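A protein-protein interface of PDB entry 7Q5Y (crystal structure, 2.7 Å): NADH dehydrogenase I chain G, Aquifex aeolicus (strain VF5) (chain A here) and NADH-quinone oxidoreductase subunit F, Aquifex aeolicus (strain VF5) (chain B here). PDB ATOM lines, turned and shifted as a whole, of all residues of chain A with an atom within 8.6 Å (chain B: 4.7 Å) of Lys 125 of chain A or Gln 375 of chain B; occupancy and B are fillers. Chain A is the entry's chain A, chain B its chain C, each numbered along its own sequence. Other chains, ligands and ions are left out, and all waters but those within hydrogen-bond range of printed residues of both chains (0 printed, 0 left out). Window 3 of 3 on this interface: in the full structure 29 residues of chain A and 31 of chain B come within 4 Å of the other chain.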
ATOM      1  N   LYS A  89     -14.427  -4.409  23.764  1.00  0.00           N
ATOM      2  CA  LYS A  89     -14.914  -5.445  22.858  1.00  0.00           C
ATOM      3  C   LYS A  89     -13.800  -6.442  22.551  1.00  0.00           C
ATOM      4  O   LYS A  89     -14.037  -7.653  22.500  1.00  0.00           O
ATOM      5  CB  LYS A  89     -15.460  -4.815  21.575  1.00  0.00           C
ATOM      6  CG  LYS A  89     -16.656  -3.908  21.847  1.00  0.00           C
ATOM      7  CD  LYS A  89     -17.411  -3.438  20.595  1.00  0.00           C
ATOM      8  CE  LYS A  89     -18.648  -2.616  21.003  1.00  0.00           C
ATOM      9  NZ  LYS A  89     -19.630  -2.380  19.902  1.00  0.00           N
ATOM     10  N   LEU A  92     -13.103  -8.608  25.871  1.00  0.00           N
ATOM     11  CA  LEU A  92     -14.164  -9.575  26.124  1.00  0.00           C
ATOM     12  C   LEU A  92     -14.187 -10.653  25.046  1.00  0.00           C
ATOM     13  O   LEU A  92     -14.410 -11.830  25.348  1.00  0.00           O
ATOM     14  CB  LEU A  92     -15.509  -8.874  26.264  1.00  0.00           C
ATOM     15  CG  LEU A  92     -15.495  -8.075  27.577  1.00  0.00           C
ATOM     16  CD1 LEU A  92     -16.548  -6.981  27.658  1.00  0.00           C
ATOM     17  CD2 LEU A  92     -15.632  -9.001  28.729  1.00  0.00           C
ATOM     18  N   GLN A  93     -13.929 -10.285  23.789  1.00  0.00           N
ATOM     19  CA  GLN A  93     -13.892 -11.309  22.747  1.00  0.00           C
ATOM     20  C   GLN A  93     -12.744 -12.284  22.984  1.00  0.00           C
ATOM     21  O   GLN A  93     -12.872 -13.495  22.736  1.00  0.00           O
ATOM     22  CB  GLN A  93     -13.748 -10.676  21.368  1.00  0.00           C
ATOM     23  CG  GLN A  93     -13.349 -11.680  20.295  1.00  0.00           C
ATOM     24  CD  GLN A  93     -14.454 -12.650  19.955  1.00  0.00           C
ATOM     25  OE1 GLN A  93     -15.122 -12.503  18.941  1.00  0.00           O
ATOM     26  NE2 GLN A  93     -14.648 -13.643  20.794  1.00  0.00           N
ATOM     27  N   MET A  96     -13.686 -14.794  25.517  1.00  0.00           N
ATOM     28  CA  MET A  96     -14.644 -15.772  24.999  1.00  0.00           C
ATOM     29  C   MET A  96     -14.090 -16.731  23.965  1.00  0.00           C
ATOM     30  O   MET A  96     -14.770 -17.699  23.630  1.00  0.00           O
ATOM     31  CB  MET A  96     -15.846 -15.047  24.403  1.00  0.00           C
ATOM     32  CG  MET A  96     -16.613 -14.289  25.460  1.00  0.00           C
ATOM     33  SD  MET A  96     -17.964 -13.364  24.764  1.00  0.00           S
ATOM     34  CE  MET A  96     -18.772 -12.706  26.206  1.00  0.00           C
ATOM     35  N   GLY A 118     -19.852  -9.399  29.095  1.00  0.00           N
ATOM     36  CA  GLY A 118     -19.803  -9.786  27.699  1.00  0.00           C
ATOM     37  C   GLY A 118     -21.045  -9.395  26.944  1.00  0.00           C
ATOM     38  O   GLY A 118     -20.997  -9.151  25.734  1.00  0.00           O
ATOM     39  N   ALA A 119     -22.168  -9.336  27.633  1.00  0.00           N
ATOM     40  CA  ALA A 119     -23.412  -8.979  26.984  1.00  0.00           C
ATOM     41  C   ALA A 119     -23.618  -7.482  26.889  1.00  0.00           C
ATOM     42  O   ALA A 119     -24.342  -7.019  26.005  1.00  0.00           O
ATOM     43  CB  ALA A 119     -24.565  -9.600  27.767  1.00  0.00           C
ATOM     44  N   GLY A 122     -19.524  -6.494  25.226  1.00  0.00           N
ATOM     45  CA  GLY A 122     -18.878  -7.417  24.344  1.00  0.00           C
ATOM     46  C   GLY A 122     -19.055  -7.117  22.881  1.00  0.00           C
ATOM     47  O   GLY A 122     -19.674  -6.123  22.475  1.00  0.00           O
ATOM     48  N   PRO A 123     -18.509  -8.025  22.066  1.00  0.00           N
ATOM     49  CA  PRO A 123     -18.583  -7.875  20.603  1.00  0.00           C
ATOM     50  C   PRO A 123     -19.982  -8.028  20.033  1.00  0.00           C
ATOM     51  O   PRO A 123     -20.209  -7.609  18.895  1.00  0.00           O
ATOM     52  CB  PRO A 123     -17.647  -8.981  20.094  1.00  0.00           C
ATOM     53  CG  PRO A 123     -17.578  -9.996  21.252  1.00  0.00           C
ATOM     54  CD  PRO A 123     -17.721  -9.197  22.502  1.00  0.00           C
ATOM     55  N   GLN A 124     -20.909  -8.639  20.765  1.00  0.00           N
ATOM     56  CA  GLN A 124     -22.302  -8.855  20.370  1.00  0.00           C
ATOM     57  C   GLN A 124     -22.459  -9.919  19.293  1.00  0.00           C
ATOM     58  O   GLN A 124     -23.573 -10.349  18.982  1.00  0.00           O
ATOM     59  CB  GLN A 124     -22.949  -7.554  19.916  1.00  0.00           C
ATOM     60  CG  GLN A 124     -22.766  -6.418  20.885  1.00  0.00           C
ATOM     61  CD  GLN A 124     -23.445  -6.700  22.200  1.00  0.00           C
ATOM     62  OE1 GLN A 124     -24.643  -6.993  22.237  1.00  0.00           O
ATOM     63  NE2 GLN A 124     -22.698  -6.571  23.296  1.00  0.00           N
ATOM     64  N   LYS A 125     -21.348 -10.359  18.732  1.00  0.00           N
ATOM     65  CA  LYS A 125     -21.355 -11.386  17.711  1.00  0.00           C
ATOM     66  C   LYS A 125     -20.006 -12.058  17.827  1.00  0.00           C
ATOM     67  O   LYS A 125     -19.121 -11.570  18.532  1.00  0.00           O
ATOM     68  CB  LYS A 125     -21.554 -10.835  16.294  1.00  0.00           C
ATOM     69  CG  LYS A 125     -20.328 -10.150  15.736  1.00  0.00           C
ATOM     70  CD  LYS A 125     -20.459  -9.869  14.256  1.00  0.00           C
ATOM     71  CE  LYS A 125     -19.316 -10.559  13.496  1.00  0.00           C
ATOM     72  NZ  LYS A 125     -19.463 -10.540  11.999  1.00  0.00           N
ATOM     73  N   GLN A 126     -19.842 -13.178  17.148  1.00  0.00           N
ATOM     74  CA  GLN A 126     -18.565 -13.864  17.196  1.00  0.00           C
ATOM     75  C   GLN A 126     -17.669 -13.337  16.080  1.00  0.00           C
ATOM     76  O   GLN A 126     -17.992 -13.485  14.897  1.00  0.00           O
ATOM     77  CB  GLN A 126     -18.738 -15.372  17.102  1.00  0.00           C
ATOM     78  CG  GLN A 126     -17.432 -16.088  17.120  1.00  0.00           C
ATOM     79  CD  GLN A 126     -17.566 -17.576  16.965  1.00  0.00           C
ATOM     80  OE1 GLN A 126     -18.159 -18.070  15.996  1.00  0.00           O
ATOM     81  NE2 GLN A 126     -17.018 -18.314  17.937  1.00  0.00           N
ATOM     82  N   ILE A 127     -16.563 -12.698  16.469  1.00  0.00           N
ATOM     83  CA  ILE A 127     -15.578 -12.164  15.533  1.00  0.00           C
ATOM     84  C   ILE A 127     -14.472 -13.182  15.264  1.00  0.00           C
ATOM     85  O   ILE A 127     -14.056 -13.358  14.117  1.00  0.00           O
ATOM     86  CB  ILE A 127     -15.008 -10.838  16.063  1.00  0.00           C
ATOM     87  CG1 ILE A 127     -16.138  -9.833  16.260  1.00  0.00           C
ATOM     88  CG2 ILE A 127     -13.922 -10.298  15.133  1.00  0.00           C
ATOM     89  CD1 ILE A 127     -15.679  -8.588  16.946  1.00  0.00           C
ATOM     90  N   VAL A 128     -13.989 -13.857  16.309  1.00  0.00           N
ATOM     91  CA  VAL A 128     -12.970 -14.903  16.212  1.00  0.00           C
ATOM     92  C   VAL A 128     -13.764 -16.207  16.148  1.00  0.00           C
ATOM     93  O   VAL A 128     -14.238 -16.702  17.183  1.00  0.00           O
ATOM     94  CB  VAL A 128     -11.999 -14.867  17.402  1.00  0.00           C
ATOM     95  CG1 VAL A 128     -10.916 -15.904  17.210  1.00  0.00           C
ATOM     96  CG2 VAL A 128     -11.428 -13.462  17.600  1.00  0.00           C
ATOM     97  N   PRO A 129     -13.933 -16.794  14.966  1.00  0.00           N
ATOM     98  CA  PRO A 129     -14.777 -17.988  14.808  1.00  0.00           C
ATOM     99  C   PRO A 129     -14.246 -19.322  15.311  1.00  0.00           C
ATOM    100  O   PRO A 129     -13.622 -20.071  14.555  1.00  0.00           O
ATOM    101  CB  PRO A 129     -14.989 -18.037  13.293  1.00  0.00           C
ATOM    102  CG  PRO A 129     -13.737 -17.464  12.754  1.00  0.00           C
ATOM    103  CD  PRO A 129     -13.297 -16.396  13.703  1.00  0.00           C
ATOM    104  N   ILE A 130     -14.503 -19.630  16.580  1.00  0.00           N
ATOM    105  CA  ILE A 130     -14.105 -20.886  17.209  1.00  0.00           C
ATOM    106  C   ILE A 130     -15.351 -21.732  17.444  1.00  0.00           C
ATOM    107  O   ILE A 130     -16.315 -21.272  18.071  1.00  0.00           O
ATOM    108  CB  ILE A 130     -13.377 -20.654  18.541  1.00  0.00           C
ATOM    109  CG1 ILE A 130     -12.195 -19.705  18.353  1.00  0.00           C
ATOM    110  CG2 ILE A 130     -12.940 -21.990  19.141  1.00  0.00           C
ATOM    111  CD1 ILE A 130     -11.157 -20.247  17.421  1.00  0.00           C
ATOM    112  N   THR B 373     -11.812 -19.149   6.343  1.00  0.00           N
ATOM    113  CA  THR B 373     -13.069 -18.614   5.854  1.00  0.00           C
ATOM    114  C   THR B 373     -13.003 -17.094   5.909  1.00  0.00           C
ATOM    115  O   THR B 373     -12.027 -16.513   6.374  1.00  0.00           O
ATOM    116  CB  THR B 373     -14.240 -19.136   6.683  1.00  0.00           C
ATOM    117  OG1 THR B 373     -14.185 -18.529   7.978  1.00  0.00           O
ATOM    118  CG2 THR B 373     -14.182 -20.652   6.818  1.00  0.00           C
ATOM    119  N   GLU B 374     -14.062 -16.439   5.430  1.00  0.00           N
ATOM    120  CA  GLU B 374     -14.086 -14.981   5.456  1.00  0.00           C
ATOM    121  C   GLU B 374     -14.071 -14.451   6.896  1.00  0.00           C
ATOM    122  O   GLU B 374     -13.405 -13.450   7.192  1.00  0.00           O
ATOM    123  CB  GLU B 374     -15.297 -14.468   4.676  1.00  0.00           C
ATOM    124  CG  GLU B 374     -15.251 -12.987   4.331  1.00  0.00           C
ATOM    125  CD  GLU B 374     -14.136 -12.611   3.343  1.00  0.00           C
ATOM    126  OE1 GLU B 374     -14.472 -12.164   2.219  1.00  0.00           O
ATOM    127  OE2 GLU B 374     -12.932 -12.749   3.676  1.00  0.00           O
ATOM    128  N   GLN B 375     -14.776 -15.117   7.817  1.00  0.00           N
ATOM    129  CA  GLN B 375     -14.760 -14.629   9.189  1.00  0.00           C
ATOM    130  C   GLN B 375     -13.387 -14.854   9.816  1.00  0.00           C
ATOM    131  O   GLN B 375     -12.929 -14.036  10.624  1.00  0.00           O
ATOM    132  CB  GLN B 375     -15.873 -15.295  10.008  1.00  0.00           C
ATOM    133  CG  GLN B 375     -16.111 -14.670  11.392  1.00  0.00           C
ATOM    134  CD  GLN B 375     -16.599 -13.232  11.311  1.00  0.00           C
ATOM    135  OE1 GLN B 375     -17.490 -12.910  10.523  1.00  0.00           O
ATOM    136  NE2 GLN B 375     -15.973 -12.347  12.095  1.00  0.00           N
ATOM    137  N   ASP B 376     -12.712 -15.946   9.436  1.00  0.00           N
ATOM    138  CA  ASP B 376     -11.367 -16.212   9.931  1.00  0.00           C
ATOM    139  C   ASP B 376     -10.460 -15.030   9.617  1.00  0.00           C
ATOM    140  O   ASP B 376      -9.688 -14.578  10.471  1.00  0.00           O
ATOM    141  CB  ASP B 376     -10.817 -17.489   9.289  1.00  0.00           C
ATOM    142  CG  ASP B 376     -11.382 -18.768   9.913  1.00  0.00           C
ATOM    143  OD1 ASP B 376     -11.374 -18.893  11.161  1.00  0.00           O
ATOM    144  OD2 ASP B 376     -11.828 -19.656   9.142  1.00  0.00           O
ATOM    145  N   TRP B 377     -10.564 -14.501   8.392  1.00  0.00           N
ATOM    146  CA  TRP B 377      -9.768 -13.342   8.007  1.00  0.00           C
ATOM    147  C   TRP B 377     -10.131 -12.129   8.849  1.00  0.00           C
ATOM    148  O   TRP B 377      -9.256 -11.479   9.429  1.00  0.00           O
ATOM    149  CB  TRP B 377      -9.979 -13.018   6.531  1.00  0.00           C
ATOM    150  CG  TRP B 377      -9.234 -13.913   5.640  1.00  0.00           C
ATOM    151  CD1 TRP B 377      -9.680 -15.062   5.071  1.00  0.00           C
ATOM    152  CD2 TRP B 377      -7.877 -13.766   5.240  1.00  0.00           C
ATOM    153  NE1 TRP B 377      -8.690 -15.633   4.311  1.00  0.00           N
ATOM    154  CE2 TRP B 377      -7.569 -14.856   4.404  1.00  0.00           C
ATOM    155  CE3 TRP B 377      -6.892 -12.817   5.503  1.00  0.00           C
ATOM    156  CZ2 TRP B 377      -6.324 -15.027   3.840  1.00  0.00           C
ATOM    157  CZ3 TRP B 377      -5.664 -12.979   4.935  1.00  0.00           C
ATOM    158  CH2 TRP B 377      -5.386 -14.075   4.110  1.00  0.00           C
ATOM    159  N   GLU B 378     -11.422 -11.802   8.926  1.00  0.00           N
ATOM    160  CA  GLU B 378     -11.836 -10.654   9.721  1.00  0.00           C
ATOM    161  C   GLU B 378     -11.358 -10.795  11.158  1.00  0.00           C
ATOM    162  O   GLU B 378     -10.922  -9.816  11.776  1.00  0.00           O
ATOM    163  CB  GLU B 378     -13.351 -10.507   9.657  1.00  0.00           C
ATOM    164  CG  GLU B 378     -13.902  -9.351  10.450  1.00  0.00           C
ATOM    165  CD  GLU B 378     -15.416  -9.373  10.478  1.00  0.00           C
ATOM    166  OE1 GLU B 378     -16.014  -9.457   9.386  1.00  0.00           O
ATOM    167  OE2 GLU B 378     -16.009  -9.323  11.581  1.00  0.00           O
ATOM    168  N   GLY B 379     -11.400 -12.019  11.694  1.00  0.00           N
ATOM    169  CA  GLY B 379     -10.945 -12.239  13.058  1.00  0.00           C
ATOM    170  C   GLY B 379      -9.444 -12.078  13.186  1.00  0.00           C
ATOM    171  O   GLY B 379      -8.954 -11.503  14.162  1.00  0.00           O
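Printed residues of chain B that touch a printed residue of chain A: Gln 375, Asp 376, Glu 378 and Gly 379. Hydrophobic or aromatic side chains of chain A that line the printed part of chain B: Pro 129. Among the printed residues, Asp or Glu carboxylates within 4 Å of a Lys or Arg side-chain nitrogen of the other chain: Lys 125 of chain A with Glu 378 of chain B (3.7 Å).
The side-chain amino group (NZ) of Lys 125 of chain A sits at hydrogen-bond distance from the side-chain amide oxygen (OE1) of Gln 375 of chain B, at 3.4 Å. O of Ile 127 of chain A lies within hydrogen-bond range of NE2 of Gln 375 of chain B, 3.0 Å away. The side-chain carboxylate (OE2) of Glu 378 of chain B lies within salt-bridge range of the side-chain amino group (NZ) of Lys 125 of chain A, at 3.7 Å.
Of chain B, only Gln 375 (3.4 Å) and Glu 378 (3.7 Å) come within 4 Å of Lys 125 of chain A. Of the printed residues of chain B, Gln 126 of chain A touches Gln 375. Printed residues of chain B within 4 Å of Ile 127 of chain A: Gln 375 and Gly 379. Gln 375 of chain B touches just these residues of chain A: Lys 125, Gln 126, Ile 127 and Pro 129. Of the printed residues of chain A, Glu 378 of chain B touches Lys 125 (3.7 Å). Of the printed residues of chain A, Gly 379 of chain B touches Ile 127.
Gln 375 of chain B touches Gln 126 of chain A. CA of Gly 379 of chain B touches O of Ile 127 of chain A (3.5 Å). Gln 375 of chain B touches Pro 129 of chain A (O to CD, 3.9 Å). CG of Pro 129 of chain A touches OD1 of Asp 376 of chain B, at 3.2 Å.
N of Ile 127 of chain A is in hydrogen-bond range of OE1 of Gln 93 of chain A (2.9 Å). O of Val 128 of chain A sits close to NE2 of Gln 126 of chain A (3.3 Å). OG1 of Thr 373 of chain B lies close to N of Gln 375 of chain B (3.5 Å). OE2 of Glu 378 of chain B lies within hydrogen-bond range of NE2 of Gln 375 of chain B (3.1 Å). The side-chain carboxylate of Asp 376 of chain B lies within hydrogen-bond range of the backbone NH of Thr 373 of chain B (2.8 Å). The backbone carbonyl oxygen of Ile 130 of chain A is in hydrogen-bond range of the side-chain amide nitrogen of Gln 126 of chain A (3.0 Å).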
